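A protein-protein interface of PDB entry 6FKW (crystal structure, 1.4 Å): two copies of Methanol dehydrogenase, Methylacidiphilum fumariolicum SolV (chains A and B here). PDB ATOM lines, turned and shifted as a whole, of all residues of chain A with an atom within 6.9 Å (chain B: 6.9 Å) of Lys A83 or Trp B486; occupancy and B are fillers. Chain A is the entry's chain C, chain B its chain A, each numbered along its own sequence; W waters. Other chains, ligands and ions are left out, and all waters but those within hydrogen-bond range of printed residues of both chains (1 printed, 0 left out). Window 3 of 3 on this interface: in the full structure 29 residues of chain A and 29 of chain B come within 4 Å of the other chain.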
ATOM      1  N   ALA A  43     -22.298  10.941 -32.539  1.00  0.00           N
ATOM      2  CA  ALA A  43     -22.875  10.593 -31.252  1.00  0.00           C
ATOM      3  C   ALA A  43     -23.911   9.494 -31.409  1.00  0.00           C
ATOM      4  O   ALA A  43     -23.898   8.510 -30.681  1.00  0.00           O
ATOM      5  CB  ALA A  43     -23.510  11.818 -30.624  1.00  0.00           C
ATOM      6  N   ASP A  79     -37.494  11.044 -28.192  1.00  0.00           N
ATOM      7  CA  ASP A  79     -37.335  11.543 -26.827  1.00  0.00           C
ATOM      8  C   ASP A  79     -35.843  11.577 -26.505  1.00  0.00           C
ATOM      9  O   ASP A  79     -35.228  10.534 -26.297  1.00  0.00           O
ATOM     10  CB  ASP A  79     -38.086  10.622 -25.857  1.00  0.00           C
ATOM     11  CG  ASP A  79     -37.990  11.069 -24.410  1.00  0.00           C
ATOM     12  OD1 ASP A  79     -37.181  11.966 -24.101  1.00  0.00           O
ATOM     13  OD2 ASP A  79     -38.736  10.508 -23.578  1.00  0.00           O
ATOM     14  N   LEU A  80     -35.274  12.779 -26.462  1.00  0.00           N
ATOM     15  CA  LEU A  80     -33.827  12.946 -26.293  1.00  0.00           C
ATOM     16  C   LEU A  80     -33.340  12.749 -24.863  1.00  0.00           C
ATOM     17  O   LEU A  80     -32.139  12.859 -24.613  1.00  0.00           O
ATOM     18  CB  LEU A  80     -33.386  14.325 -26.785  1.00  0.00           C
ATOM     19  CG  LEU A  80     -33.706  14.647 -28.247  1.00  0.00           C
ATOM     20  CD1 LEU A  80     -33.218  16.043 -28.590  1.00  0.00           C
ATOM     21  CD2 LEU A  80     -33.096  13.616 -29.190  1.00  0.00           C
ATOM     22  N   THR A  81     -34.247  12.463 -23.929  1.00  0.00           N
ATOM     23  CA  THR A  81     -33.849  12.138 -22.557  1.00  0.00           C
ATOM     24  C   THR A  81     -33.481  10.666 -22.377  1.00  0.00           C
ATOM     25  O   THR A  81     -33.028  10.281 -21.302  1.00  0.00           O
ATOM     26  CB  THR A  81     -34.962  12.471 -21.536  1.00  0.00           C
ATOM     27  OG1 THR A  81     -36.077  11.585 -21.719  1.00  0.00           O
ATOM     28  CG2 THR A  81     -35.414  13.909 -21.672  1.00  0.00           C
ATOM     29  N   GLN A  82     -33.664   9.845 -23.415  1.00  0.00           N
ATOM     30  CA  GLN A  82     -33.563   8.386 -23.269  1.00  0.00           C
ATOM     31  C   GLN A  82     -32.223   7.771 -23.695  1.00  0.00           C
ATOM     32  O   GLN A  82     -32.150   6.567 -23.961  1.00  0.00           O
ATOM     33  CB  GLN A  82     -34.722   7.713 -24.011  1.00  0.00           C
ATOM     34  CG  GLN A  82     -36.091   8.101 -23.466  1.00  0.00           C
ATOM     35  CD  GLN A  82     -36.244   7.766 -21.995  1.00  0.00           C
ATOM     36  OE1 GLN A  82     -36.414   8.654 -21.153  1.00  0.00           O
ATOM     37  NE2 GLN A  82     -36.179   6.482 -21.675  1.00  0.00           N
ATOM     38  N   LYS A  83     -31.176   8.592 -23.758  1.00  0.00           N
ATOM     39  CA  LYS A  83     -29.794   8.116 -23.698  1.00  0.00           C
ATOM     40  C   LYS A  83     -29.391   7.141 -24.818  1.00  0.00           C
ATOM     41  O   LYS A  83     -29.168   5.956 -24.549  1.00  0.00           O
ATOM     42  CB  LYS A  83     -29.544   7.456 -22.333  1.00  0.00           C
ATOM     43  CG  LYS A  83     -29.849   8.357 -21.138  1.00  0.00           C
ATOM     44  CD  LYS A  83     -29.649   7.641 -19.809  1.00  0.00           C
ATOM     45  CE  LYS A  83     -28.241   7.083 -19.638  1.00  0.00           C
ATOM     46  NZ  LYS A  83     -27.176   8.093 -19.893  1.00  0.00           N
ATOM     47  N   PRO A  84     -29.281   7.612 -26.062  1.00  0.00           N
ATOM     48  CA  PRO A  84     -29.411   9.020 -26.447  1.00  0.00           C
ATOM     49  C   PRO A  84     -30.815   9.423 -26.901  1.00  0.00           C
ATOM     50  O   PRO A  84     -31.146  10.611 -26.895  1.00  0.00           O
ATOM     51  CB  PRO A  84     -28.453   9.129 -27.630  1.00  0.00           C
ATOM     52  CG  PRO A  84     -28.504   7.780 -28.263  1.00  0.00           C
ATOM     53  CD  PRO A  84     -28.687   6.800 -27.141  1.00  0.00           C
ATOM     54  N   TYR A  85     -31.626   8.448 -27.302  1.00  0.00           N
ATOM     55  CA  TYR A  85     -32.997   8.718 -27.708  1.00  0.00           C
ATOM     56  C   TYR A  85     -33.834   7.454 -27.663  1.00  0.00           C
ATOM     57  O   TYR A  85     -33.302   6.345 -27.661  1.00  0.00           O
ATOM     58  CB  TYR A  85     -33.056   9.328 -29.118  1.00  0.00           C
ATOM     59  CG  TYR A  85     -32.719   8.368 -30.244  1.00  0.00           C
ATOM     60  CD1 TYR A  85     -33.700   7.569 -30.830  1.00  0.00           C
ATOM     61  CD2 TYR A  85     -31.420   8.263 -30.728  1.00  0.00           C
ATOM     62  CE1 TYR A  85     -33.390   6.690 -31.862  1.00  0.00           C
ATOM     63  CE2 TYR A  85     -31.104   7.391 -31.755  1.00  0.00           C
ATOM     64  CZ  TYR A  85     -32.087   6.609 -32.318  1.00  0.00           C
ATOM     65  OH  TYR A  85     -31.759   5.746 -33.341  1.00  0.00           O
ATOM     66  N   ALA A  86     -35.147   7.647 -27.623  1.00  0.00           N
ATOM     67  CA  ALA A  86     -36.112   6.578 -27.841  1.00  0.00           C
ATOM     68  C   ALA A  86     -37.153   7.111 -28.810  1.00  0.00           C
ATOM     69  O   ALA A  86     -37.385   8.318 -28.858  1.00  0.00           O
ATOM     70  CB  ALA A  86     -36.763   6.166 -26.535  1.00  0.00           C
ATOM     71  N   GLU B 462     -30.117  -9.678 -22.849  1.00  0.00           N
ATOM     72  CA  GLU B 462     -30.406  -8.667 -23.855  1.00  0.00           C
ATOM     73  C   GLU B 462     -31.903  -8.597 -24.009  1.00  0.00           C
ATOM     74  O   GLU B 462     -32.574  -9.632 -24.014  1.00  0.00           O
ATOM     75  CB  GLU B 462     -29.746  -9.035 -25.186  1.00  0.00           C
ATOM     76  CG  GLU B 462     -28.254  -8.752 -25.203  1.00  0.00           C
ATOM     77  CD  GLU B 462     -27.917  -7.281 -25.364  1.00  0.00           C
ATOM     78  OE1 GLU B 462     -26.709  -6.965 -25.408  1.00  0.00           O
ATOM     79  OE2 GLU B 462     -28.836  -6.430 -25.447  1.00  0.00           O
ATOM     80  N   TYR B 480     -20.698  -7.197 -31.268  1.00  0.00           N
ATOM     81  CA  TYR B 480     -21.982  -7.644 -31.820  1.00  0.00           C
ATOM     82  C   TYR B 480     -22.982  -6.508 -31.756  1.00  0.00           C
ATOM     83  O   TYR B 480     -22.787  -5.542 -31.030  1.00  0.00           O
ATOM     84  CB  TYR B 480     -22.512  -8.876 -31.076  1.00  0.00           C
ATOM     85  CG  TYR B 480     -22.978  -8.630 -29.650  1.00  0.00           C
ATOM     86  CD1 TYR B 480     -22.078  -8.661 -28.591  1.00  0.00           C
ATOM     87  CD2 TYR B 480     -24.316  -8.373 -29.358  1.00  0.00           C
ATOM     88  CE1 TYR B 480     -22.497  -8.441 -27.287  1.00  0.00           C
ATOM     89  CE2 TYR B 480     -24.743  -8.151 -28.056  1.00  0.00           C
ATOM     90  CZ  TYR B 480     -23.828  -8.185 -27.019  1.00  0.00           C
ATOM     91  OH  TYR B 480     -24.249  -7.968 -25.728  1.00  0.00           O
ATOM     92  N   GLY B 481     -24.056  -6.632 -32.528  1.00  0.00           N
ATOM     93  CA  GLY B 481     -25.123  -5.637 -32.543  1.00  0.00           C
ATOM     94  C   GLY B 481     -26.409  -6.145 -31.934  1.00  0.00           C
ATOM     95  O   GLY B 481     -26.623  -7.356 -31.835  1.00  0.00           O
ATOM     96  N   THR B 482     -27.266  -5.211 -31.525  1.00  0.00           N
ATOM     97  CA  THR B 482     -28.585  -5.540 -30.989  1.00  0.00           C
ATOM     98  C   THR B 482     -29.672  -5.075 -31.944  1.00  0.00           C
ATOM     99  O   THR B 482     -29.441  -4.220 -32.806  1.00  0.00           O
ATOM    100  CB  THR B 482     -28.815  -4.890 -29.616  1.00  0.00           C
ATOM    101  OG1 THR B 482     -28.949  -3.474 -29.772  1.00  0.00           O
ATOM    102  CG2 THR B 482     -27.662  -5.199 -28.674  1.00  0.00           C
ATOM    103  N   MET B 483     -30.864  -5.640 -31.774  1.00  0.00           N
ATOM    104  CA  MET B 483     -31.968  -5.365 -32.685  1.00  0.00           C
ATOM    105  C   MET B 483     -32.610  -3.999 -32.502  1.00  0.00           C
ATOM    106  O   MET B 483     -33.426  -3.596 -33.327  1.00  0.00           O
ATOM    107  CB  MET B 483     -33.019  -6.478 -32.607  1.00  0.00           C
ATOM    108  CG  MET B 483     -32.469  -7.809 -33.097  1.00  0.00           C
ATOM    109  SD  MET B 483     -33.741  -9.040 -33.425  1.00  0.00           S
ATOM    110  CE  MET B 483     -34.419  -8.396 -34.955  1.00  0.00           C
ATOM    111  N   ASP B 484     -32.254  -3.277 -31.441  1.00  0.00           N
ATOM    112  CA  ASP B 484     -32.656  -1.873 -31.353  1.00  0.00           C
ATOM    113  C   ASP B 484     -31.514  -0.906 -31.683  1.00  0.00           C
ATOM    114  O   ASP B 484     -31.591   0.283 -31.363  1.00  0.00           O
ATOM    115  CB  ASP B 484     -33.316  -1.554 -30.010  1.00  0.00           C
ATOM    116  CG  ASP B 484     -32.391  -1.738 -28.837  1.00  0.00           C
ATOM    117  OD1 ASP B 484     -31.418  -2.510 -28.944  1.00  0.00           O
ATOM    118  OD2 ASP B 484     -32.649  -1.102 -27.794  1.00  0.00           O
ATOM    119  N   GLY B 485     -30.462  -1.417 -32.322  1.00  0.00           N
ATOM    120  CA  GLY B 485     -29.477  -0.573 -32.984  1.00  0.00           C
ATOM    121  C   GLY B 485     -28.177  -0.320 -32.245  1.00  0.00           C
ATOM    122  O   GLY B 485     -27.337   0.441 -32.729  1.00  0.00           O
ATOM    123  N   TRP B 486     -27.990  -0.944 -31.086  1.00  0.00           N
ATOM    124  CA  TRP B 486     -26.738  -0.762 -30.346  1.00  0.00           C
ATOM    125  C   TRP B 486     -25.647  -1.681 -30.866  1.00  0.00           C
ATOM    126  O   TRP B 486     -25.830  -2.891 -30.921  1.00  0.00           O
ATOM    127  CB  TRP B 486     -26.942  -1.020 -28.857  1.00  0.00           C
ATOM    128  CG  TRP B 486     -27.701   0.050 -28.171  1.00  0.00           C
ATOM    129  CD1 TRP B 486     -29.041   0.081 -27.923  1.00  0.00           C
ATOM    130  CD2 TRP B 486     -27.163   1.262 -27.637  1.00  0.00           C
ATOM    131  NE1 TRP B 486     -29.374   1.240 -27.263  1.00  0.00           N
ATOM    132  CE2 TRP B 486     -28.237   1.985 -27.076  1.00  0.00           C
ATOM    133  CE3 TRP B 486     -25.878   1.809 -27.580  1.00  0.00           C
ATOM    134  CZ2 TRP B 486     -28.062   3.223 -26.466  1.00  0.00           C
ATOM    135  CZ3 TRP B 486     -25.706   3.043 -26.972  1.00  0.00           C
ATOM    136  CH2 TRP B 486     -26.792   3.734 -26.423  1.00  0.00           C
ATOM    137  N   PHE B 487     -24.518  -1.088 -31.240  1.00  0.00           N
ATOM    138  CA  PHE B 487     -23.323  -1.841 -31.575  1.00  0.00           C
ATOM    139  C   PHE B 487     -22.399  -1.800 -30.363  1.00  0.00           C
ATOM    140  O   PHE B 487     -22.115  -0.728 -29.841  1.00  0.00           O
ATOM    141  CB  PHE B 487     -22.661  -1.242 -32.814  1.00  0.00           C
ATOM    142  CG  PHE B 487     -21.562  -2.089 -33.402  1.00  0.00           C
ATOM    143  CD1 PHE B 487     -21.723  -3.460 -33.574  1.00  0.00           C
ATOM    144  CD2 PHE B 487     -20.362  -1.509 -33.789  1.00  0.00           C
ATOM    145  CE1 PHE B 487     -20.706  -4.231 -34.119  1.00  0.00           C
ATOM    146  CE2 PHE B 487     -19.346  -2.275 -34.334  1.00  0.00           C
ATOM    147  CZ  PHE B 487     -19.519  -3.639 -34.498  1.00  0.00           C
ATOM    148  N   LYS B 488     -21.949  -2.976 -29.933  1.00  0.00           N
ATOM    149  CA  LYS B 488     -21.276  -3.145 -28.649  1.00  0.00           C
ATOM    150  C   LYS B 488     -19.973  -3.910 -28.777  1.00  0.00           C
ATOM    151  O   LYS B 488     -19.847  -4.815 -29.601  1.00  0.00           O
ATOM    152  CB  LYS B 488     -22.181  -3.921 -27.689  1.00  0.00           C
ATOM    153  CG  LYS B 488     -23.513  -3.264 -27.380  1.00  0.00           C
ATOM    154  CD  LYS B 488     -24.327  -4.155 -26.455  1.00  0.00           C
ATOM    155  CE  LYS B 488     -25.653  -3.516 -26.085  1.00  0.00           C
ATOM    156  NZ  LYS B 488     -26.318  -4.256 -24.978  1.00  0.00           N
ATOM    157  N   GLN B 500     -20.021   1.167 -26.636  1.00  0.00           N
ATOM    158  CA  GLN B 500     -21.229   0.992 -27.438  1.00  0.00           C
ATOM    159  C   GLN B 500     -21.707   2.294 -28.058  1.00  0.00           C
ATOM    160  O   GLN B 500     -21.456   3.378 -27.541  1.00  0.00           O
ATOM    161  CB  GLN B 500     -22.349   0.371 -26.607  1.00  0.00           C
ATOM    162  CG  GLN B 500     -22.813   1.225 -25.444  1.00  0.00           C
ATOM    163  CD  GLN B 500     -23.911   0.563 -24.637  1.00  0.00           C
ATOM    164  OE1 GLN B 500     -24.094  -0.655 -24.692  1.00  0.00           O
ATOM    165  NE2 GLN B 500     -24.651   1.363 -23.885  1.00  0.00           N
ATOM    166  N   GLN B 501     -22.409   2.161 -29.179  1.00  0.00           N
ATOM    167  CA  GLN B 501     -22.982   3.306 -29.876  1.00  0.00           C
ATOM    168  C   GLN B 501     -24.309   2.895 -30.484  1.00  0.00           C
ATOM    169  O   GLN B 501     -24.444   1.770 -30.971  1.00  0.00           O
ATOM    170  CB  GLN B 501     -22.042   3.786 -30.971  1.00  0.00           C
ATOM    171  CG  GLN B 501     -22.515   5.055 -31.663  1.00  0.00           C
ATOM    172  CD  GLN B 501     -21.429   5.724 -32.478  1.00  0.00           C
ATOM    173  OE1 GLN B 501     -20.255   5.698 -32.111  1.00  0.00           O
ATOM    174  NE2 GLN B 501     -21.816   6.331 -33.598  1.00  0.00           N
ATOM    175  N   LYS B 502     -25.275   3.813 -30.448  1.00  0.00           N
ATOM    176  CA  LYS B 502     -26.592   3.553 -31.030  1.00  0.00           C
ATOM    177  C   LYS B 502     -26.605   3.981 -32.493  1.00  0.00           C
ATOM    178  O   LYS B 502     -26.411   5.161 -32.813  1.00  0.00           O
ATOM    179  CB  LYS B 502     -27.713   4.268 -30.263  1.00  0.00           C
ATOM    180  CG  LYS B 502     -29.098   3.762 -30.667  1.00  0.00           C
ATOM    181  CD  LYS B 502     -30.225   4.263 -29.786  1.00  0.00           C
ATOM    182  CE  LYS B 502     -31.554   3.659 -30.234  1.00  0.00           C
ATOM    183  NZ  LYS B 502     -32.699   4.117 -29.400  1.00  0.00           N
ATOM    184  N   LEU B 503     -26.841   3.002 -33.360  1.00  0.00           N
ATOM    185  CA  LEU B 503     -26.901   3.199 -34.804  1.00  0.00           C
ATOM    186  C   LEU B 503     -28.354   3.371 -35.237  1.00  0.00           C
ATOM    187  O   LEU B 503     -29.266   3.298 -34.414  1.00  0.00           O
ATOM    188  CB  LEU B 503     -26.254   2.009 -35.517  1.00  0.00           C
ATOM    189  CG  LEU B 503     -24.866   1.616 -34.998  1.00  0.00           C
ATOM    190  CD1 LEU B 503     -24.221   0.590 -35.909  1.00  0.00           C
ATOM    191  CD2 LEU B 503     -24.000   2.858 -34.877  1.00  0.00           C
ATOM    192  N   SER B 505     -30.604   1.760 -37.178  1.00  0.00           N
ATOM    193  CA  SER B 505     -31.575   0.677 -37.315  1.00  0.00           C
ATOM    194  C   SER B 505     -31.030  -0.547 -36.595  1.00  0.00           C
ATOM    195  O   SER B 505     -29.815  -0.671 -36.401  1.00  0.00           O
ATOM    196  CB  SER B 505     -31.803   0.360 -38.801  1.00  0.00           C
ATOM    197  OG  SER B 505     -32.794  -0.642 -38.999  1.00  0.00           O
ATOM    198  N   GLY B 506     -31.916  -1.450 -36.198  1.00  0.00           N
ATOM    199  CA  GLY B 506     -31.503  -2.711 -35.591  1.00  0.00           C
ATOM    200  C   GLY B 506     -30.450  -3.412 -36.416  1.00  0.00           C
ATOM    201  O   GLY B 506     -30.472  -3.368 -37.648  1.00  0.00           O
ATOM    202  N   ILE B 507     -29.520  -4.062 -35.729  1.00  0.00           N
ATOM    203  CA  ILE B 507     -28.383  -4.697 -36.371  1.00  0.00           C
ATOM    204  C   ILE B 507     -28.623  -6.189 -36.444  1.00  0.00           C
ATOM    205  O   ILE B 507     -28.732  -6.853 -35.415  1.00  0.00           O
ATOM    206  CB  ILE B 507     -27.090  -4.426 -35.574  1.00  0.00           C
ATOM    207  CG1 ILE B 507     -26.784  -2.926 -35.586  1.00  0.00           C
ATOM    208  CG2 ILE B 507     -25.923  -5.221 -36.152  1.00  0.00           C
ATOM    209  CD1 ILE B 507     -25.816  -2.490 -34.503  1.00  0.00           C
HETATM  210  O   HOH W   1     -24.959   6.316 -29.225  1.00  0.00           O
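The side-chain amino group (NZ) of Lys B502 is in hydrogen-bond range of the backbone carbonyl oxygen (O) of Tyr A85 (2.9 Å).
OG1 of Thr B482 sits at hydrogen-bond distance from N of Trp B486, 3.0 Å away.
N of Leu B503 lies within hydrogen-bond range of O of Gly B485.
N of Phe B487 sits at hydrogen-bond distance from O of Gln B501.
Ala A43 touches Gln B501.
CZ2 of Trp B486 touches O of Lys A83, 3.5 Å away.
Pro A84 touches Trp B486.
Pro A84 touches Lys B502 (CD to CD, 3.97 Å).
O of Leu B503 touches OH of Tyr A85, 3.7 Å away.
Printed residues of chain B within 4 Å of Lys A83: Trp B486.
Printed residues of chain B within 4 Å of Tyr A85: Lys B502 and Leu B503.
No residue of chain A comes within 4 Å of Gly B485.
Trp B486 touches just these residues of chain A: Lys A83 (3.5 Å) and Pro A84 (3.7 Å).
Gln B500 touches none of the printed residues of chain A.
Of the printed residues of chain A, Leu B503 touches Tyr A85 (3.7 Å).
The nearest printed residue of chain A that does not touch Gln B501 is Pro A84 (6.8 Å).
Hydrophobic or aromatic side chains of chain A within 4 Å of the printed part of chain B: Pro A84 and Tyr A85.
Among the printed residues, 6 pairs touch across the chains.
No position is printed for both chains.
Of the 6 pairs that touch across the chains among the printed residues, none has its exchanged pair printed and touching as well.
Water W1 bridges the backbone NH of Lys B502 (2.8 Å) and the backbone carbonyl oxygen of Ala A43 (2.8 Å).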
